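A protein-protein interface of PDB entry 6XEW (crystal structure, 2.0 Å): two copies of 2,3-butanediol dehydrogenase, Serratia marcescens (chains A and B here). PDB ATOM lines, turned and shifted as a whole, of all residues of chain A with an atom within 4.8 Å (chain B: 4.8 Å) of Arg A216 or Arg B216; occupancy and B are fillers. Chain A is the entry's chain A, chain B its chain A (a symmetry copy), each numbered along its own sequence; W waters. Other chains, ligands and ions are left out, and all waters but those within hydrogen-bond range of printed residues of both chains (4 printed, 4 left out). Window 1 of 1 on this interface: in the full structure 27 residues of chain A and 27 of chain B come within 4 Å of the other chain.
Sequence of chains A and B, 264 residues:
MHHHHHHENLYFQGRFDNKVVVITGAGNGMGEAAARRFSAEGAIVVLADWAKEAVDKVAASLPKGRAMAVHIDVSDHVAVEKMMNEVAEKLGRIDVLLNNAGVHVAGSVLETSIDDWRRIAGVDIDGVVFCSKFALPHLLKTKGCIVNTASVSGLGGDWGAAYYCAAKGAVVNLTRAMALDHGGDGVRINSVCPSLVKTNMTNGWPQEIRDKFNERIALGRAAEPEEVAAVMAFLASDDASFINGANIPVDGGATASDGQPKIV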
ATOM      1  N   TRP A 159       2.924   9.922 -32.248  1.00  0.00           N
ATOM      2  CA  TRP A 159       3.737  11.159 -32.154  1.00  0.00           C
ATOM      3  C   TRP A 159       4.756  11.135 -33.281  1.00  0.00           C
ATOM      4  O   TRP A 159       5.595  10.198 -33.270  1.00  0.00           O
ATOM      5  CB  TRP A 159       4.482  11.213 -30.815  1.00  0.00           C
ATOM      6  CG  TRP A 159       3.670  11.539 -29.610  1.00  0.00           C
ATOM      7  CD1 TRP A 159       3.493  12.759 -29.017  1.00  0.00           C
ATOM      8  CD2 TRP A 159       2.986  10.588 -28.781  1.00  0.00           C
ATOM      9  NE1 TRP A 159       2.728  12.632 -27.886  1.00  0.00           N
ATOM     10  CE2 TRP A 159       2.412  11.313 -27.709  1.00  0.00           C
ATOM     11  CE3 TRP A 159       2.786   9.207 -28.859  1.00  0.00           C
ATOM     12  CZ2 TRP A 159       1.654  10.687 -26.726  1.00  0.00           C
ATOM     13  CZ3 TRP A 159       2.068   8.589 -27.862  1.00  0.00           C
ATOM     14  CH2 TRP A 159       1.497   9.321 -26.829  1.00  0.00           C
ATOM     15  N   LYS A 212      11.719   1.310 -26.042  1.00  0.00           N
ATOM     16  CA  LYS A 212      10.365   1.753 -25.623  1.00  0.00           C
ATOM     17  C   LYS A 212       9.292   0.842 -26.262  1.00  0.00           C
ATOM     18  O   LYS A 212       8.278   0.576 -25.588  1.00  0.00           O
ATOM     19  CB  LYS A 212      10.152   3.236 -25.935  1.00  0.00           C
ATOM     20  CG  LYS A 212      10.961   4.200 -25.094  1.00  0.00           C
ATOM     21  CD  LYS A 212      10.452   5.611 -25.191  1.00  0.00           C
ATOM     22  CE  LYS A 212      11.464   6.646 -24.742  1.00  0.00           C
ATOM     23  NZ  LYS A 212      10.850   7.660 -23.845  1.00  0.00           N
ATOM     24  N   PHE A 213       9.511   0.354 -27.485  1.00  0.00           N
ATOM     25  CA  PHE A 213       8.587  -0.594 -28.167  1.00  0.00           C
ATOM     26  C   PHE A 213       8.469  -1.907 -27.378  1.00  0.00           C
ATOM     27  O   PHE A 213       7.347  -2.463 -27.275  1.00  0.00           O
ATOM     28  CB  PHE A 213       8.979  -0.873 -29.621  1.00  0.00           C
ATOM     29  CG  PHE A 213       8.297   0.022 -30.624  1.00  0.00           C
ATOM     30  CD1 PHE A 213       7.009  -0.250 -31.048  1.00  0.00           C
ATOM     31  CD2 PHE A 213       8.917   1.167 -31.103  1.00  0.00           C
ATOM     32  CE1 PHE A 213       6.381   0.561 -31.983  1.00  0.00           C
ATOM     33  CE2 PHE A 213       8.285   1.993 -32.024  1.00  0.00           C
ATOM     34  CZ  PHE A 213       7.011   1.680 -32.466  1.00  0.00           C
ATOM     35  N   ASN A 214       9.577  -2.383 -26.820  1.00  0.00           N
ATOM     36  CA  ASN A 214       9.590  -3.622 -26.001  1.00  0.00           C
ATOM     37  C   ASN A 214       8.784  -3.398 -24.729  1.00  0.00           C
ATOM     38  O   ASN A 214       8.305  -4.364 -24.177  1.00  0.00           O
ATOM     39  CB  ASN A 214      11.012  -4.130 -25.777  1.00  0.00           C
ATOM     40  CG  ASN A 214      11.648  -4.566 -27.074  1.00  0.00           C
ATOM     41  OD1 ASN A 214      10.953  -4.749 -28.066  1.00  0.00           O
ATOM     42  ND2 ASN A 214      12.968  -4.718 -27.085  1.00  0.00           N
ATOM     43  N   GLU A 215       8.624  -2.143 -24.285  1.00  0.00           N
ATOM     44  CA  GLU A 215       7.774  -1.785 -23.113  1.00  0.00           C
ATOM     45  C   GLU A 215       6.296  -1.708 -23.548  1.00  0.00           C
ATOM     46  O   GLU A 215       5.430  -2.273 -22.834  1.00  0.00           O
ATOM     47  CB  GLU A 215       8.268  -0.487 -22.455  1.00  0.00           C
ATOM     48  CG  GLU A 215       7.569  -0.157 -21.139  1.00  0.00           C
ATOM     49  CD  GLU A 215       8.118   1.016 -20.326  1.00  0.00           C
ATOM     50  OE1 GLU A 215       7.296   1.792 -19.776  1.00  0.00           O
ATOM     51  OE2 GLU A 215       9.365   1.132 -20.203  1.00  0.00           O
ATOM     52  N   ARG A 216       6.010  -1.031 -24.665  1.00  0.00           N
ATOM     53  CA  ARG A 216       4.622  -0.750 -25.123  1.00  0.00           C
ATOM     54  C   ARG A 216       3.962  -1.996 -25.751  1.00  0.00           C
ATOM     55  O   ARG A 216       2.714  -2.046 -25.779  1.00  0.00           O
ATOM     56  CB  ARG A 216       4.627   0.422 -26.099  1.00  0.00           C
ATOM     57  CG  ARG A 216       4.986   1.761 -25.461  1.00  0.00           C
ATOM     58  CD  ARG A 216       4.178   2.116 -24.230  1.00  0.00           C
ATOM     59  NE  ARG A 216       2.751   1.988 -24.466  1.00  0.00           N
ATOM     60  CZ  ARG A 216       1.790   2.120 -23.556  1.00  0.00           C
ATOM     61  NH1 ARG A 216       0.530   1.909 -23.913  1.00  0.00           N
ATOM     62  NH2 ARG A 216       2.070   2.375 -22.289  1.00  0.00           N
ATOM     63  N   ILE A 217       4.758  -2.931 -26.252  1.00  0.00           N
ATOM     64  CA  ILE A 217       4.303  -4.238 -26.812  1.00  0.00           C
ATOM     65  C   ILE A 217       4.452  -5.285 -25.705  1.00  0.00           C
ATOM     66  O   ILE A 217       5.568  -5.540 -25.259  1.00  0.00           O
ATOM     67  CB  ILE A 217       5.090  -4.611 -28.080  1.00  0.00           C
ATOM     68  CG1 ILE A 217       4.840  -3.621 -29.227  1.00  0.00           C
ATOM     69  CG2 ILE A 217       4.787  -6.054 -28.502  1.00  0.00           C
ATOM     70  CD1 ILE A 217       5.667  -3.921 -30.475  1.00  0.00           C
ATOM     71  N   ALA A 218       3.349  -5.838 -25.236  1.00  0.00           N
ATOM     72  CA  ALA A 218       3.347  -6.727 -24.064  1.00  0.00           C
ATOM     73  C   ALA A 218       4.159  -8.006 -24.348  1.00  0.00           C
ATOM     74  O   ALA A 218       4.719  -8.570 -23.379  1.00  0.00           O
ATOM     75  CB  ALA A 218       1.905  -7.045 -23.715  1.00  0.00           C
ATOM     76  N   ALA A 254      -0.193  -4.005 -28.592  1.00  0.00           N
ATOM     77  CA  ALA A 254       0.006  -2.540 -28.569  1.00  0.00           C
ATOM     78  C   ALA A 254      -1.343  -1.821 -28.443  1.00  0.00           C
ATOM     79  O   ALA A 254      -1.460  -0.946 -27.562  1.00  0.00           O
ATOM     80  CB  ALA A 254       0.743  -2.095 -29.798  1.00  0.00           C
ATOM     81  N   SER A 257      -3.926  -1.782 -25.266  1.00  0.00           N
ATOM     82  CA  SER A 257      -3.682  -0.809 -24.181  1.00  0.00           C
ATOM     83  C   SER A 257      -4.536   0.435 -24.433  1.00  0.00           C
ATOM     84  O   SER A 257      -4.714   0.823 -25.641  1.00  0.00           O
ATOM     85  CB  SER A 257      -2.216  -0.450 -24.102  1.00  0.00           C
ATOM     86  OG  SER A 257      -1.968   0.575 -23.137  1.00  0.00           O
ATOM     87  N   GLY A 259      -3.315   3.256 -23.675  1.00  0.00           N
ATOM     88  CA  GLY A 259      -2.229   4.244 -23.819  1.00  0.00           C
ATOM     89  C   GLY A 259      -1.523   4.560 -22.481  1.00  0.00           C
ATOM     90  O   GLY A 259      -0.443   5.175 -22.480  1.00  0.00           O
ATOM     91  N   GLN A 260      -2.113   4.153 -21.368  1.00  0.00           N
ATOM     92  CA  GLN A 260      -1.553   4.466 -20.035  1.00  0.00           C
ATOM     93  C   GLN A 260      -0.298   3.627 -19.866  1.00  0.00           C
ATOM     94  O   GLN A 260      -0.178   2.538 -20.433  1.00  0.00           O
ATOM     95  CB  GLN A 260      -2.591   4.244 -18.942  1.00  0.00           C
ATOM     96  CG  GLN A 260      -3.789   5.190 -19.069  1.00  0.00           C
ATOM     97  CD  GLN A 260      -4.701   5.198 -17.868  1.00  0.00           C
ATOM     98  OE1 GLN A 260      -5.266   6.230 -17.509  1.00  0.00           O
ATOM     99  NE2 GLN A 260      -4.869   4.036 -17.250  1.00  0.00           N
ATOM    100  N   PRO A 261       0.669   4.125 -19.067  1.00  0.00           N
ATOM    101  CA  PRO A 261       1.865   3.349 -18.742  1.00  0.00           C
ATOM    102  C   PRO A 261       1.458   2.234 -17.780  1.00  0.00           C
ATOM    103  O   PRO A 261       0.381   2.267 -17.302  1.00  0.00           O
ATOM    104  CB  PRO A 261       2.772   4.361 -18.047  1.00  0.00           C
ATOM    105  CG  PRO A 261       1.809   5.358 -17.429  1.00  0.00           C
ATOM    106  CD  PRO A 261       0.613   5.427 -18.374  1.00  0.00           C
ATOM    107  N   TRP B 159      -1.825  -2.672 -17.864  1.00  0.00           N
ATOM    108  CA  TRP B 159      -0.939  -3.615 -17.140  1.00  0.00           C
ATOM    109  C   TRP B 159      -1.209  -3.462 -15.652  1.00  0.00           C
ATOM    110  O   TRP B 159      -0.966  -2.338 -15.143  1.00  0.00           O
ATOM    111  CB  TRP B 159       0.534  -3.285 -17.411  1.00  0.00           C
ATOM    112  CG  TRP B 159       1.068  -3.660 -18.750  1.00  0.00           C
ATOM    113  CD1 TRP B 159       1.751  -4.792 -19.099  1.00  0.00           C
ATOM    114  CD2 TRP B 159       1.040  -2.832 -19.922  1.00  0.00           C
ATOM    115  NE1 TRP B 159       2.132  -4.731 -20.416  1.00  0.00           N
ATOM    116  CE2 TRP B 159       1.721  -3.538 -20.942  1.00  0.00           C
ATOM    117  CE3 TRP B 159       0.485  -1.581 -20.207  1.00  0.00           C
ATOM    118  CZ2 TRP B 159       1.856  -3.020 -22.226  1.00  0.00           C
ATOM    119  CZ3 TRP B 159       0.656  -1.058 -21.468  1.00  0.00           C
ATOM    120  CH2 TRP B 159       1.311  -1.775 -22.460  1.00  0.00           C
ATOM    121  N   LYS B 212       5.698   8.761 -16.213  1.00  0.00           N
ATOM    122  CA  LYS B 212       5.347   8.023 -17.453  1.00  0.00           C
ATOM    123  C   LYS B 212       3.981   8.513 -17.988  1.00  0.00           C
ATOM    124  O   LYS B 212       3.830   8.578 -19.223  1.00  0.00           O
ATOM    125  CB  LYS B 212       5.390   6.511 -17.222  1.00  0.00           C
ATOM    126  CG  LYS B 212       6.769   5.925 -17.009  1.00  0.00           C
ATOM    127  CD  LYS B 212       6.785   4.429 -17.151  1.00  0.00           C
ATOM    128  CE  LYS B 212       8.003   3.779 -16.525  1.00  0.00           C
ATOM    129  NZ  LYS B 212       8.606   2.764 -17.427  1.00  0.00           N
ATOM    130  N   PHE B 213       3.043   8.876 -17.111  1.00  0.00           N
ATOM    131  CA  PHE B 213       1.722   9.437 -17.510  1.00  0.00           C
ATOM    132  C   PHE B 213       1.896  10.759 -18.272  1.00  0.00           C
ATOM    133  O   PHE B 213       1.165  10.995 -19.268  1.00  0.00           O
ATOM    134  CB  PHE B 213       0.764   9.618 -16.328  1.00  0.00           C
ATOM    135  CG  PHE B 213      -0.155   8.446 -16.097  1.00  0.00           C
ATOM    136  CD1 PHE B 213      -1.306   8.296 -16.848  1.00  0.00           C
ATOM    137  CD2 PHE B 213       0.156   7.461 -15.169  1.00  0.00           C
ATOM    138  CE1 PHE B 213      -2.165   7.229 -16.628  1.00  0.00           C
ATOM    139  CE2 PHE B 213      -0.690   6.381 -14.960  1.00  0.00           C
ATOM    140  CZ  PHE B 213      -1.859   6.271 -15.695  1.00  0.00           C
ATOM    141  N   ASN B 214       2.839  11.590 -17.843  1.00  0.00           N
ATOM    142  CA  ASN B 214       3.132  12.881 -18.514  1.00  0.00           C
ATOM    143  C   ASN B 214       3.693  12.615 -19.905  1.00  0.00           C
ATOM    144  O   ASN B 214       3.569  13.477 -20.747  1.00  0.00           O
ATOM    145  CB  ASN B 214       3.995  13.785 -17.638  1.00  0.00           C
ATOM    146  CG  ASN B 214       3.258  14.203 -16.389  1.00  0.00           C
ATOM    147  OD1 ASN B 214       2.044  14.057 -16.317  1.00  0.00           O
ATOM    148  ND2 ASN B 214       3.980  14.708 -15.395  1.00  0.00           N
ATOM    149  N   GLU B 215       4.282  11.434 -20.142  1.00  0.00           N
ATOM    150  CA  GLU B 215       4.777  11.015 -21.485  1.00  0.00           C
ATOM    151  C   GLU B 215       3.602  10.479 -22.327  1.00  0.00           C
ATOM    152  O   GLU B 215       3.486  10.875 -23.514  1.00  0.00           O
ATOM    153  CB  GLU B 215       5.924  10.001 -21.352  1.00  0.00           C
ATOM    154  CG  GLU B 215       6.611   9.668 -22.675  1.00  0.00           C
ATOM    155  CD  GLU B 215       7.873   8.809 -22.615  1.00  0.00           C
ATOM    156  OE1 GLU B 215       8.025   7.916 -23.488  1.00  0.00           O
ATOM    157  OE2 GLU B 215       8.729   9.056 -21.726  1.00  0.00           O
ATOM    158  N   ARG B 216       2.767   9.609 -21.750  1.00  0.00           N
ATOM    159  CA  ARG B 216       1.682   8.901 -22.482  1.00  0.00           C
ATOM    160  C   ARG B 216       0.476   9.824 -22.754  1.00  0.00           C
ATOM    161  O   ARG B 216      -0.290   9.526 -23.695  1.00  0.00           O
ATOM    162  CB  ARG B 216       1.262   7.656 -21.707  1.00  0.00           C
ATOM    163  CG  ARG B 216       2.325   6.564 -21.660  1.00  0.00           C
ATOM    164  CD  ARG B 216       2.890   6.166 -23.008  1.00  0.00           C
ATOM    165  NE  ARG B 216       1.839   5.866 -23.965  1.00  0.00           N
ATOM    166  CZ  ARG B 216       2.007   5.597 -25.257  1.00  0.00           C
ATOM    167  NH1 ARG B 216       0.940   5.406 -26.020  1.00  0.00           N
ATOM    168  NH2 ARG B 216       3.209   5.598 -25.811  1.00  0.00           N
ATOM    169  N   ILE B 217       0.303  10.867 -21.952  1.00  0.00           N
ATOM    170  CA  ILE B 217      -0.749  11.913 -22.118  1.00  0.00           C
ATOM    171  C   ILE B 217      -0.104  13.097 -22.843  1.00  0.00           C
ATOM    172  O   ILE B 217       0.820  13.704 -22.306  1.00  0.00           O
ATOM    173  CB  ILE B 217      -1.359  12.316 -20.765  1.00  0.00           C
ATOM    174  CG1 ILE B 217      -2.109  11.153 -20.100  1.00  0.00           C
ATOM    175  CG2 ILE B 217      -2.253  13.553 -20.919  1.00  0.00           C
ATOM    176  CD1 ILE B 217      -2.660  11.502 -18.718  1.00  0.00           C
ATOM    177  N   ALA B 218      -0.543  13.383 -24.055  1.00  0.00           N
ATOM    178  CA  ALA B 218       0.106  14.385 -24.914  1.00  0.00           C
ATOM    179  C   ALA B 218       0.014  15.787 -24.283  1.00  0.00           C
ATOM    180  O   ALA B 218       0.927  16.607 -24.543  1.00  0.00           O
ATOM    181  CB  ALA B 218      -0.557  14.338 -26.277  1.00  0.00           C
ATOM    182  N   ALA B 254      -4.675  10.224 -24.393  1.00  0.00           N
ATOM    183  CA  ALA B 254      -4.139   8.886 -24.063  1.00  0.00           C
ATOM    184  C   ALA B 254      -4.635   7.848 -25.077  1.00  0.00           C
ATOM    185  O   ALA B 254      -3.791   7.098 -25.609  1.00  0.00           O
ATOM    186  CB  ALA B 254      -4.524   8.502 -22.664  1.00  0.00           C
ATOM    187  N   SER B 257      -3.711   7.522 -29.053  1.00  0.00           N
ATOM    188  CA  SER B 257      -2.473   6.805 -29.425  1.00  0.00           C
ATOM    189  C   SER B 257      -2.825   5.353 -29.752  1.00  0.00           C
ATOM    190  O   SER B 257      -3.744   4.775 -29.073  1.00  0.00           O
ATOM    191  CB  SER B 257      -1.457   6.875 -28.308  1.00  0.00           C
ATOM    192  OG  SER B 257      -0.294   6.094 -28.594  1.00  0.00           O
ATOM    193  N   GLY B 259      -0.758   3.100 -28.928  1.00  0.00           N
ATOM    194  CA  GLY B 259       0.038   2.437 -27.877  1.00  0.00           C
ATOM    195  C   GLY B 259       1.558   2.507 -28.143  1.00  0.00           C
ATOM    196  O   GLY B 259       2.360   2.217 -27.238  1.00  0.00           O
ATOM    197  N   GLN B 260       1.951   2.880 -29.351  1.00  0.00           N
ATOM    198  CA  GLN B 260       3.382   2.911 -29.726  1.00  0.00           C
ATOM    199  C   GLN B 260       4.016   4.076 -28.986  1.00  0.00           C
ATOM    200  O   GLN B 260       3.354   5.072 -28.679  1.00  0.00           O
ATOM    201  CB  GLN B 260       3.548   2.982 -31.239  1.00  0.00           C
ATOM    202  CG  GLN B 260       3.009   1.736 -31.948  1.00  0.00           C
ATOM    203  CD  GLN B 260       3.395   1.636 -33.402  1.00  0.00           C
ATOM    204  OE1 GLN B 260       3.621   0.546 -33.925  1.00  0.00           O
ATOM    205  NE2 GLN B 260       3.450   2.779 -34.075  1.00  0.00           N
ATOM    206  N   PRO B 261       5.328   3.972 -28.687  1.00  0.00           N
ATOM    207  CA  PRO B 261       6.063   5.081 -28.082  1.00  0.00           C
ATOM    208  C   PRO B 261       6.253   6.159 -29.148  1.00  0.00           C
ATOM    209  O   PRO B 261       5.997   5.896 -30.268  1.00  0.00           O
ATOM    210  CB  PRO B 261       7.402   4.458 -27.696  1.00  0.00           C
ATOM    211  CG  PRO B 261       7.583   3.326 -28.690  1.00  0.00           C
ATOM    212  CD  PRO B 261       6.181   2.808 -28.996  1.00  0.00           C
HETATM  213  O   HOH W   1      -1.486   0.339 -17.760  1.00  0.00           O
HETATM  214  O   HOH W   2       3.247  14.912 -26.185  1.00  0.00           O
HETATM  215  O   HOH W   3       4.359  -6.537 -20.794  1.00  0.00           O
HETATM  216  O   HOH W   4       4.027   7.161 -31.658  1.00  0.00           O
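NE of Arg B216 lies within hydrogen-bond range of O of Gly A259, 2.8 Å away. The guanidinium group (NE) of Arg A216 sits at hydrogen-bond distance from the backbone carbonyl oxygen (O) of Gly B259. The side-chain amino group (NZ) of Lys B212 is in salt-bridge range of the side-chain carboxylate (OE1) of Glu A215. The side-chain amino group (NZ) of Lys A212 lies within salt-bridge range of the side-chain carboxylate (OE1) of Glu B215, 2.9 Å away.
The guanidinium group of Arg B216 lies within hydrogen-bond range of the side-chain hydroxyl of Ser B257, at 2.9 Å. The backbone NH of Gly B259 lies within hydrogen-bond range of the side-chain hydroxyl of Ser B257 (3.0 Å). N of Gly A259 sits at hydrogen-bond distance from OG of Ser A257 (3.0 Å). NH1 of Arg A216 sits at hydrogen-bond distance from OG of Ser A257, 2.9 Å away. The backbone carbonyl oxygen (O) of Gln A260 lies within hydrogen-bond range of the guanidinium group (NH2) of Arg A216. NH2 of Arg B216 is in hydrogen-bond range of O of Gln B260, at 2.9 Å.
CZ2 of Trp A159 touches O of Glu B215, at 3.7 Å. Trp A159 touches Arg B216. CG of Pro B261 touches CD2 of Phe A213, at 3.5 Å. Trp B159 touches Glu A215 (CZ2 to O, 3.7 Å). O of Arg A216 touches CH2 of Trp B159 (3.6 Å). OG of Ser A257 touches CZ3 of Trp B159, at 3.5 Å. Gly A259 touches Ala B254. Trp B159 touches Gln A260 (CZ3 to O, 3.8 Å). Pro A261 touches Lys B212 (CB to CB, 3.5 Å). CG of Pro A261 touches CD2 of Phe B213 (3.5 Å).
Of the printed residues of chain B, Trp A159 touches Glu B215, Arg B216, Ser B257 and Gln B260. Of the printed residues of chain B, Arg A216 touches Trp B159 (3.6 Å), Arg B216 (3.8 Å), Gly B259 (2.8 Å) and Pro B261 (3.9 Å). Ile A217 touches none of the printed residues of chain B. Arg B216 touches just these residues of chain A: Trp A159, Arg A216, Gly A259 and Pro A261. Printed residues of chain A within 4 Å of Ala B254: Gly A259 (3.7 Å). The nearest printed residue of chain A that does not touch Arg B216 is Gln A260 (4.3 Å).
Hydrophobic or aromatic side chains of chain B that line the printed part of chain A: Trp B159, Phe B213 and Pro B261. Printed residues of chain A that touch a printed residue of chain B: Trp A159, Lys A212, Phe A213, Glu A215, Arg A216, Ala A254, Ser A257, Gly A259, Gln A260 and Pro A261. Hydrophobic or aromatic side chains of chain A that line the printed part of chain B: Trp A159, Phe A213 and Pro A261. Among the printed residues, 23 pairs touch across the chains.
Trp A159 touches Gln B260, and with the chains exchanged Gln A260 touches Trp B159. Lys A212 touches Pro B261, and with the chains exchanged Pro A261 touches Lys B212. Arg A216 touches Gly B259, and with the chains exchanged Gly A259 touches Arg B216. Arg A216 touches Pro B261, and with the chains exchanged Pro A261 touches Arg B216.
Water W1 lies within hydrogen-bond range of the backbone carbonyl oxygen (O) of Pro A261 (2.7 Å) and the backbone NH (N) of Trp B159 (3.0 Å). Water W4 lies within hydrogen-bond range of O of Pro B261 (2.7 Å) and N of Trp A159 (3.0 Å). Water W2 bridges NE1 of Trp A159 (2.9 Å) and O of Ala B218 (3.3 Å). Water W3 bridges the indole nitrogen (NE1) of Trp B159 (2.9 Å) and the backbone carbonyl oxygen (O) of Ala A218 (3.3 Å).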
